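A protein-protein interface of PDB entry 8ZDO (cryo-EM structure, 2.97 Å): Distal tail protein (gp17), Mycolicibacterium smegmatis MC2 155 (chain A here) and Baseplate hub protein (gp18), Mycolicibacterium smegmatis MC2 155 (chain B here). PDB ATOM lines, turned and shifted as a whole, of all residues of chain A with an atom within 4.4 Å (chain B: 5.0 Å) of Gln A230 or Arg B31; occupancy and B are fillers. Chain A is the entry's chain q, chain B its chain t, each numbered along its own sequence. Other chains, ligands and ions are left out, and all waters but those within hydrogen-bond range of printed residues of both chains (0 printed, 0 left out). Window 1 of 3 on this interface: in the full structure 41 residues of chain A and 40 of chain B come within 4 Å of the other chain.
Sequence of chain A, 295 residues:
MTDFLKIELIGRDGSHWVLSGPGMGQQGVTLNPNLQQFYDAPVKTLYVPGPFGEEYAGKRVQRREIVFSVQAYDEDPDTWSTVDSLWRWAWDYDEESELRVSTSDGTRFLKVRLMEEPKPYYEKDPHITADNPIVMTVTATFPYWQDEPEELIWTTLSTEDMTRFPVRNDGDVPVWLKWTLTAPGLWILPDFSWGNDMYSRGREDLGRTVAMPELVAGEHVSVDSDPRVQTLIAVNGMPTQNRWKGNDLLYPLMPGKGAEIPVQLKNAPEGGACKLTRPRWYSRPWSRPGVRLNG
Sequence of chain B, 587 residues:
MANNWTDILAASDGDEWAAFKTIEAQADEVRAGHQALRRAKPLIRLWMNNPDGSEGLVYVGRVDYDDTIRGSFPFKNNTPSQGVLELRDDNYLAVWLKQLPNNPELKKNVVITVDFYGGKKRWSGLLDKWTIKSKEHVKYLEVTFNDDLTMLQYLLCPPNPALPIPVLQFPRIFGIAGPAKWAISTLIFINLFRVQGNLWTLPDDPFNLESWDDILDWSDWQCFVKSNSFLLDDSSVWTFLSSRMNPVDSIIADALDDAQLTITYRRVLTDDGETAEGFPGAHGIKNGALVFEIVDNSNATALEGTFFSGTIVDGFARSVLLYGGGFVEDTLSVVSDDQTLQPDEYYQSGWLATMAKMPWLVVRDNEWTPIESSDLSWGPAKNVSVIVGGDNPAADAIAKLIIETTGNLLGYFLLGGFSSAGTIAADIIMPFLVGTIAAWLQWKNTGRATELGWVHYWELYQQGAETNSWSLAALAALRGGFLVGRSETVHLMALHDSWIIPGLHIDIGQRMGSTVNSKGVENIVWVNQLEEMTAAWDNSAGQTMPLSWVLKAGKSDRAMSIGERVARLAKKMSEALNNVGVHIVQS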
ATOM      1  N   SER A 222      13.141 -17.920  27.094  1.00  0.00           N
ATOM      2  CA  SER A 222      12.088 -16.962  27.377  1.00  0.00           C
ATOM      3  C   SER A 222      11.185 -17.559  28.446  1.00  0.00           C
ATOM      4  O   SER A 222      10.755 -18.715  28.333  1.00  0.00           O
ATOM      5  CB  SER A 222      11.298 -16.620  26.115  1.00  0.00           C
ATOM      6  OG  SER A 222      10.559 -17.736  25.658  1.00  0.00           O
ATOM      7  N   ASP A 224       7.858 -16.829  30.256  1.00  0.00           N
ATOM      8  CA  ASP A 224       6.617 -16.065  30.222  1.00  0.00           C
ATOM      9  C   ASP A 224       5.704 -16.557  31.335  1.00  0.00           C
ATOM     10  O   ASP A 224       5.339 -17.736  31.362  1.00  0.00           O
ATOM     11  CB  ASP A 224       5.935 -16.202  28.862  1.00  0.00           C
ATOM     12  CG  ASP A 224       5.006 -15.045  28.556  1.00  0.00           C
ATOM     13  OD1 ASP A 224       4.634 -14.313  29.496  1.00  0.00           O
ATOM     14  OD2 ASP A 224       4.643 -14.870  27.375  1.00  0.00           O
ATOM     15  N   VAL A 229       0.586 -19.462  27.803  1.00  0.00           N
ATOM     16  CA  VAL A 229       1.761 -19.969  27.115  1.00  0.00           C
ATOM     17  C   VAL A 229       2.619 -20.739  28.111  1.00  0.00           C
ATOM     18  O   VAL A 229       2.575 -20.485  29.318  1.00  0.00           O
ATOM     19  CB  VAL A 229       2.539 -18.796  26.472  1.00  0.00           C
ATOM     20  CG1 VAL A 229       3.808 -19.258  25.834  1.00  0.00           C
ATOM     21  CG2 VAL A 229       1.672 -18.076  25.450  1.00  0.00           C
ATOM     22  N   GLN A 230       3.397 -21.695  27.601  1.00  0.00           N
ATOM     23  CA  GLN A 230       4.326 -22.434  28.447  1.00  0.00           C
ATOM     24  C   GLN A 230       5.379 -21.494  29.023  1.00  0.00           C
ATOM     25  O   GLN A 230       5.807 -20.542  28.368  1.00  0.00           O
ATOM     26  CB  GLN A 230       4.996 -23.551  27.651  1.00  0.00           C
ATOM     27  CG  GLN A 230       5.834 -24.489  28.494  1.00  0.00           C
ATOM     28  CD  GLN A 230       6.457 -25.602  27.686  1.00  0.00           C
ATOM     29  OE1 GLN A 230       6.203 -25.733  26.492  1.00  0.00           O
ATOM     30  NE2 GLN A 230       7.277 -26.416  28.337  1.00  0.00           N
ATOM     31  N   THR A 231       5.799 -21.772  30.258  1.00  0.00           N
ATOM     32  CA  THR A 231       6.649 -20.832  30.984  1.00  0.00           C
ATOM     33  C   THR A 231       8.041 -20.741  30.368  1.00  0.00           C
ATOM     34  O   THR A 231       8.457 -19.671  29.913  1.00  0.00           O
ATOM     35  CB  THR A 231       6.739 -21.235  32.456  1.00  0.00           C
ATOM     36  OG1 THR A 231       5.424 -21.496  32.959  1.00  0.00           O
ATOM     37  CG2 THR A 231       7.363 -20.118  33.270  1.00  0.00           C
ATOM     38  N   LEU A 232       8.776 -21.852  30.357  1.00  0.00           N
ATOM     39  CA  LEU A 232      10.137 -21.903  29.835  1.00  0.00           C
ATOM     40  C   LEU A 232      10.109 -22.378  28.391  1.00  0.00           C
ATOM     41  O   LEU A 232       9.598 -23.466  28.106  1.00  0.00           O
ATOM     42  CB  LEU A 232      11.013 -22.849  30.659  1.00  0.00           C
ATOM     43  CG  LEU A 232      11.613 -22.471  32.009  1.00  0.00           C
ATOM     44  CD1 LEU A 232      12.348 -23.661  32.584  1.00  0.00           C
ATOM     45  CD2 LEU A 232      12.572 -21.332  31.837  1.00  0.00           C
ATOM     46  N   ILE A 233      10.664 -21.578  27.485  1.00  0.00           N
ATOM     47  CA  ILE A 233      10.912 -22.023  26.116  1.00  0.00           C
ATOM     48  C   ILE A 233      12.316 -21.600  25.720  1.00  0.00           C
ATOM     49  O   ILE A 233      12.638 -20.409  25.748  1.00  0.00           O
ATOM     50  CB  ILE A 233       9.873 -21.474  25.125  1.00  0.00           C
ATOM     51  CG1 ILE A 233       8.526 -22.166  25.330  1.00  0.00           C
ATOM     52  CG2 ILE A 233      10.349 -21.652  23.699  1.00  0.00           C
ATOM     53  CD1 ILE A 233       8.568 -23.656  25.091  1.00  0.00           C
ATOM     54  N   GLN A 241      12.105 -26.710  30.578  1.00  0.00           N
ATOM     55  CA  GLN A 241      11.133 -26.923  31.642  1.00  0.00           C
ATOM     56  C   GLN A 241      11.142 -28.353  32.157  1.00  0.00           C
ATOM     57  O   GLN A 241      10.750 -28.587  33.304  1.00  0.00           O
ATOM     58  CB  GLN A 241       9.734 -26.548  31.156  1.00  0.00           C
ATOM     59  CG  GLN A 241       8.707 -26.440  32.261  1.00  0.00           C
ATOM     60  CD  GLN A 241       7.687 -25.362  31.997  1.00  0.00           C
ATOM     61  OE1 GLN A 241       7.954 -24.407  31.273  1.00  0.00           O
ATOM     62  NE2 GLN A 241       6.511 -25.504  32.588  1.00  0.00           N
ATOM     63  N   ALA B  27      12.251 -17.647  20.167  1.00  0.00           N
ATOM     64  CA  ALA B  27      11.333 -18.256  21.126  1.00  0.00           C
ATOM     65  C   ALA B  27       9.917 -18.315  20.568  1.00  0.00           C
ATOM     66  O   ALA B  27       9.201 -19.302  20.771  1.00  0.00           O
ATOM     67  CB  ALA B  27      11.362 -17.484  22.443  1.00  0.00           C
ATOM     68  N   ASP B  28       9.501 -17.266  19.859  1.00  0.00           N
ATOM     69  CA  ASP B  28       8.171 -17.237  19.265  1.00  0.00           C
ATOM     70  C   ASP B  28       8.017 -18.315  18.204  1.00  0.00           C
ATOM     71  O   ASP B  28       6.960 -18.943  18.102  1.00  0.00           O
ATOM     72  CB  ASP B  28       7.892 -15.859  18.669  1.00  0.00           C
ATOM     73  CG  ASP B  28       7.548 -14.827  19.725  1.00  0.00           C
ATOM     74  OD1 ASP B  28       7.043 -15.219  20.797  1.00  0.00           O
ATOM     75  OD2 ASP B  28       7.783 -13.626  19.482  1.00  0.00           O
ATOM     76  N   GLU B  29       9.055 -18.539  17.395  1.00  0.00           N
ATOM     77  CA  GLU B  29       8.955 -19.584  16.381  1.00  0.00           C
ATOM     78  C   GLU B  29       8.914 -20.969  17.015  1.00  0.00           C
ATOM     79  O   GLU B  29       8.200 -21.851  16.523  1.00  0.00           O
ATOM     80  CB  GLU B  29      10.101 -19.470  15.371  1.00  0.00           C
ATOM     81  CG  GLU B  29      11.410 -20.111  15.790  1.00  0.00           C
ATOM     82  CD  GLU B  29      12.551 -19.788  14.849  1.00  0.00           C
ATOM     83  OE1 GLU B  29      12.336 -19.014  13.892  1.00  0.00           O
ATOM     84  OE2 GLU B  29      13.667 -20.306  15.069  1.00  0.00           O
ATOM     85  N   VAL B  30       9.635 -21.175  18.121  1.00  0.00           N
ATOM     86  CA  VAL B  30       9.531 -22.453  18.823  1.00  0.00           C
ATOM     87  C   VAL B  30       8.122 -22.647  19.381  1.00  0.00           C
ATOM     88  O   VAL B  30       7.532 -23.732  19.268  1.00  0.00           O
ATOM     89  CB  VAL B  30      10.594 -22.553  19.929  1.00  0.00           C
ATOM     90  CG1 VAL B  30      10.403 -23.829  20.729  1.00  0.00           C
ATOM     91  CG2 VAL B  30      11.986 -22.502  19.330  1.00  0.00           C
ATOM     92  N   ARG B  31       7.557 -21.598  19.984  1.00  0.00           N
ATOM     93  CA  ARG B  31       6.203 -21.696  20.521  1.00  0.00           C
ATOM     94  C   ARG B  31       5.190 -21.958  19.414  1.00  0.00           C
ATOM     95  O   ARG B  31       4.236 -22.722  19.599  1.00  0.00           O
ATOM     96  CB  ARG B  31       5.837 -20.419  21.279  1.00  0.00           C
ATOM     97  CG  ARG B  31       6.655 -20.150  22.533  1.00  0.00           C
ATOM     98  CD  ARG B  31       6.162 -18.886  23.221  1.00  0.00           C
ATOM     99  NE  ARG B  31       7.179 -18.228  24.032  1.00  0.00           N
ATOM    100  CZ  ARG B  31       7.457 -18.529  25.293  1.00  0.00           C
ATOM    101  NH1 ARG B  31       6.866 -19.534  25.913  1.00  0.00           N
ATOM    102  NH2 ARG B  31       8.354 -17.801  25.949  1.00  0.00           N
ATOM    103  N   ALA B  32       5.374 -21.316  18.258  1.00  0.00           N
ATOM    104  CA  ALA B  32       4.473 -21.527  17.130  1.00  0.00           C
ATOM    105  C   ALA B  32       4.570 -22.951  16.608  1.00  0.00           C
ATOM    106  O   ALA B  32       3.554 -23.548  16.235  1.00  0.00           O
ATOM    107  CB  ALA B  32       4.781 -20.525  16.019  1.00  0.00           C
ATOM    108  N   GLY B  33       5.780 -23.505  16.556  1.00  0.00           N
ATOM    109  CA  GLY B  33       5.917 -24.903  16.188  1.00  0.00           C
ATOM    110  C   GLY B  33       5.191 -25.822  17.148  1.00  0.00           C
ATOM    111  O   GLY B  33       4.521 -26.773  16.732  1.00  0.00           O
ATOM    112  N   HIS B  34       5.305 -25.544  18.450  1.00  0.00           N
ATOM    113  CA  HIS B  34       4.579 -26.340  19.436  1.00  0.00           C
ATOM    114  C   HIS B  34       3.073 -26.234  19.236  1.00  0.00           C
ATOM    115  O   HIS B  34       2.354 -27.236  19.323  1.00  0.00           O
ATOM    116  CB  HIS B  34       4.953 -25.904  20.851  1.00  0.00           C
ATOM    117  CG  HIS B  34       6.291 -26.394  21.302  1.00  0.00           C
ATOM    118  ND1 HIS B  34       7.020 -25.763  22.285  1.00  0.00           N
ATOM    119  CD2 HIS B  34       7.034 -27.451  20.901  1.00  0.00           C
ATOM    120  CE1 HIS B  34       8.155 -26.410  22.472  1.00  0.00           C
ATOM    121  NE2 HIS B  34       8.189 -27.439  21.645  1.00  0.00           N
ATOM    122  N   GLN B  35       2.573 -25.025  18.977  1.00  0.00           N
ATOM    123  CA  GLN B  35       1.137 -24.846  18.792  1.00  0.00           C
ATOM    124  C   GLN B  35       0.644 -25.556  17.538  1.00  0.00           C
ATOM    125  O   GLN B  35      -0.436 -26.158  17.543  1.00  0.00           O
ATOM    126  CB  GLN B  35       0.792 -23.361  18.734  1.00  0.00           C
ATOM    127  CG  GLN B  35      -0.671 -23.089  18.451  1.00  0.00           C
ATOM    128  CD  GLN B  35      -1.044 -21.636  18.648  1.00  0.00           C
ATOM    129  OE1 GLN B  35      -0.207 -20.812  19.014  1.00  0.00           O
ATOM    130  NE2 GLN B  35      -2.309 -21.315  18.407  1.00  0.00           N
ATOM    131  N   TRP B 360       8.282 -34.109  35.245  1.00  0.00           N
ATOM    132  CA  TRP B 360       8.373 -32.657  35.182  1.00  0.00           C
ATOM    133  C   TRP B 360       7.041 -31.952  35.032  1.00  0.00           C
ATOM    134  O   TRP B 360       6.958 -30.766  35.368  1.00  0.00           O
ATOM    135  CB  TRP B 360       9.267 -32.231  34.011  1.00  0.00           C
ATOM    136  CG  TRP B 360       8.643 -32.516  32.687  1.00  0.00           C
ATOM    137  CD1 TRP B 360       8.628 -33.707  32.033  1.00  0.00           C
ATOM    138  CD2 TRP B 360       7.922 -31.595  31.864  1.00  0.00           C
ATOM    139  NE1 TRP B 360       7.951 -33.586  30.847  1.00  0.00           N
ATOM    140  CE2 TRP B 360       7.506 -32.297  30.721  1.00  0.00           C
ATOM    141  CE3 TRP B 360       7.592 -30.244  31.983  1.00  0.00           C
ATOM    142  CZ2 TRP B 360       6.779 -31.696  29.705  1.00  0.00           C
ATOM    143  CZ3 TRP B 360       6.873 -29.650  30.975  1.00  0.00           C
ATOM    144  CH2 TRP B 360       6.474 -30.374  29.848  1.00  0.00           C
ATOM    145  N   TRP B 499      -1.005 -25.574  26.684  1.00  0.00           N
ATOM    146  CA  TRP B 499       0.198 -25.905  25.936  1.00  0.00           C
ATOM    147  C   TRP B 499       0.573 -27.374  26.047  1.00  0.00           C
ATOM    148  O   TRP B 499       1.431 -27.833  25.288  1.00  0.00           O
ATOM    149  CB  TRP B 499       1.357 -25.040  26.423  1.00  0.00           C
ATOM    150  CG  TRP B 499       1.538 -25.106  27.900  1.00  0.00           C
ATOM    151  CD1 TRP B 499       0.968 -24.293  28.830  1.00  0.00           C
ATOM    152  CD2 TRP B 499       2.333 -26.048  28.623  1.00  0.00           C
ATOM    153  NE1 TRP B 499       1.364 -24.665  30.088  1.00  0.00           N
ATOM    154  CE2 TRP B 499       2.205 -25.741  29.987  1.00  0.00           C
ATOM    155  CE3 TRP B 499       3.148 -27.118  28.246  1.00  0.00           C
ATOM    156  CZ2 TRP B 499       2.858 -26.464  30.976  1.00  0.00           C
ATOM    157  CZ3 TRP B 499       3.796 -27.833  29.228  1.00  0.00           C
ATOM    158  CH2 TRP B 499       3.648 -27.504  30.578  1.00  0.00           C
ATOM    159  N   HIS B 505       4.105 -34.616  25.394  1.00  0.00           N
ATOM    160  CA  HIS B 505       4.640 -34.167  26.673  1.00  0.00           C
ATOM    161  C   HIS B 505       4.490 -35.240  27.742  1.00  0.00           C
ATOM    162  O   HIS B 505       5.402 -35.453  28.548  1.00  0.00           O
ATOM    163  CB  HIS B 505       3.943 -32.882  27.113  1.00  0.00           C
ATOM    164  CG  HIS B 505       4.508 -31.645  26.493  1.00  0.00           C
ATOM    165  ND1 HIS B 505       3.723 -30.583  26.106  1.00  0.00           N
ATOM    166  CD2 HIS B 505       5.781 -31.300  26.194  1.00  0.00           C
ATOM    167  CE1 HIS B 505       4.486 -29.634  25.597  1.00  0.00           C
ATOM    168  NE2 HIS B 505       5.740 -30.045  25.637  1.00  0.00           N
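Among the printed residues, merely in contact across the chains: Ser A222 with Ala B27, Val A229 with Arg B31, Val A229 with Trp B499, Gln A230 with Trp B499, Ile A233 with Ala B27, Ile A233 with Val B30, Ile A233 with Arg B31, Ile A233 with His B34 and Gln A241 with Trp B360.
The backbone carbonyl oxygen (O) of Gln A230 lies within hydrogen-bond range of the guanidinium group (NH1) of Arg B31, at 2.9 Å. The side-chain hydroxyl (OG) of Ser A222 sits close to the guanidinium group (NH2) of Arg B31, at 2.2 Å.
Gln A230 touches just these residues of chain B: Arg B31 (2.9 Å) and Trp B499 (3.7 Å). Arg B31 touches four residues of chain A. Of the printed residues of chain A, Trp B360 touches Gln A241. Printed residues of chain A within 4 Å of Val B30: Ile A233. Printed residues of chain B within 4 Å of Gln A241: Trp B360. Of the printed residues of chain A, Ala B27 touches Ser A222 (3.3 Å) and Ile A233 (3.9 Å). The nearest residue of chain B that does not touch Gln A230 is Trp B360 (4.2 Å). The nearest printed residue of chain B that does not touch Ile A233 is Asp B28 (5.9 Å).
Hydrophobic or aromatic side chains of chain B within 4 Å of the printed part of chain A: Ala B27, Val B30, His B34, Trp B360 and Trp B499.
The backbone NH (N) of Ser A222 sits at hydrogen-bond distance from the backbone carbonyl oxygen (O) of Ile A233. The backbone NH (N) of Leu A232 is in hydrogen-bond range of the side-chain amide oxygen (OE1) of Gln A241, 2.8 Å away.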
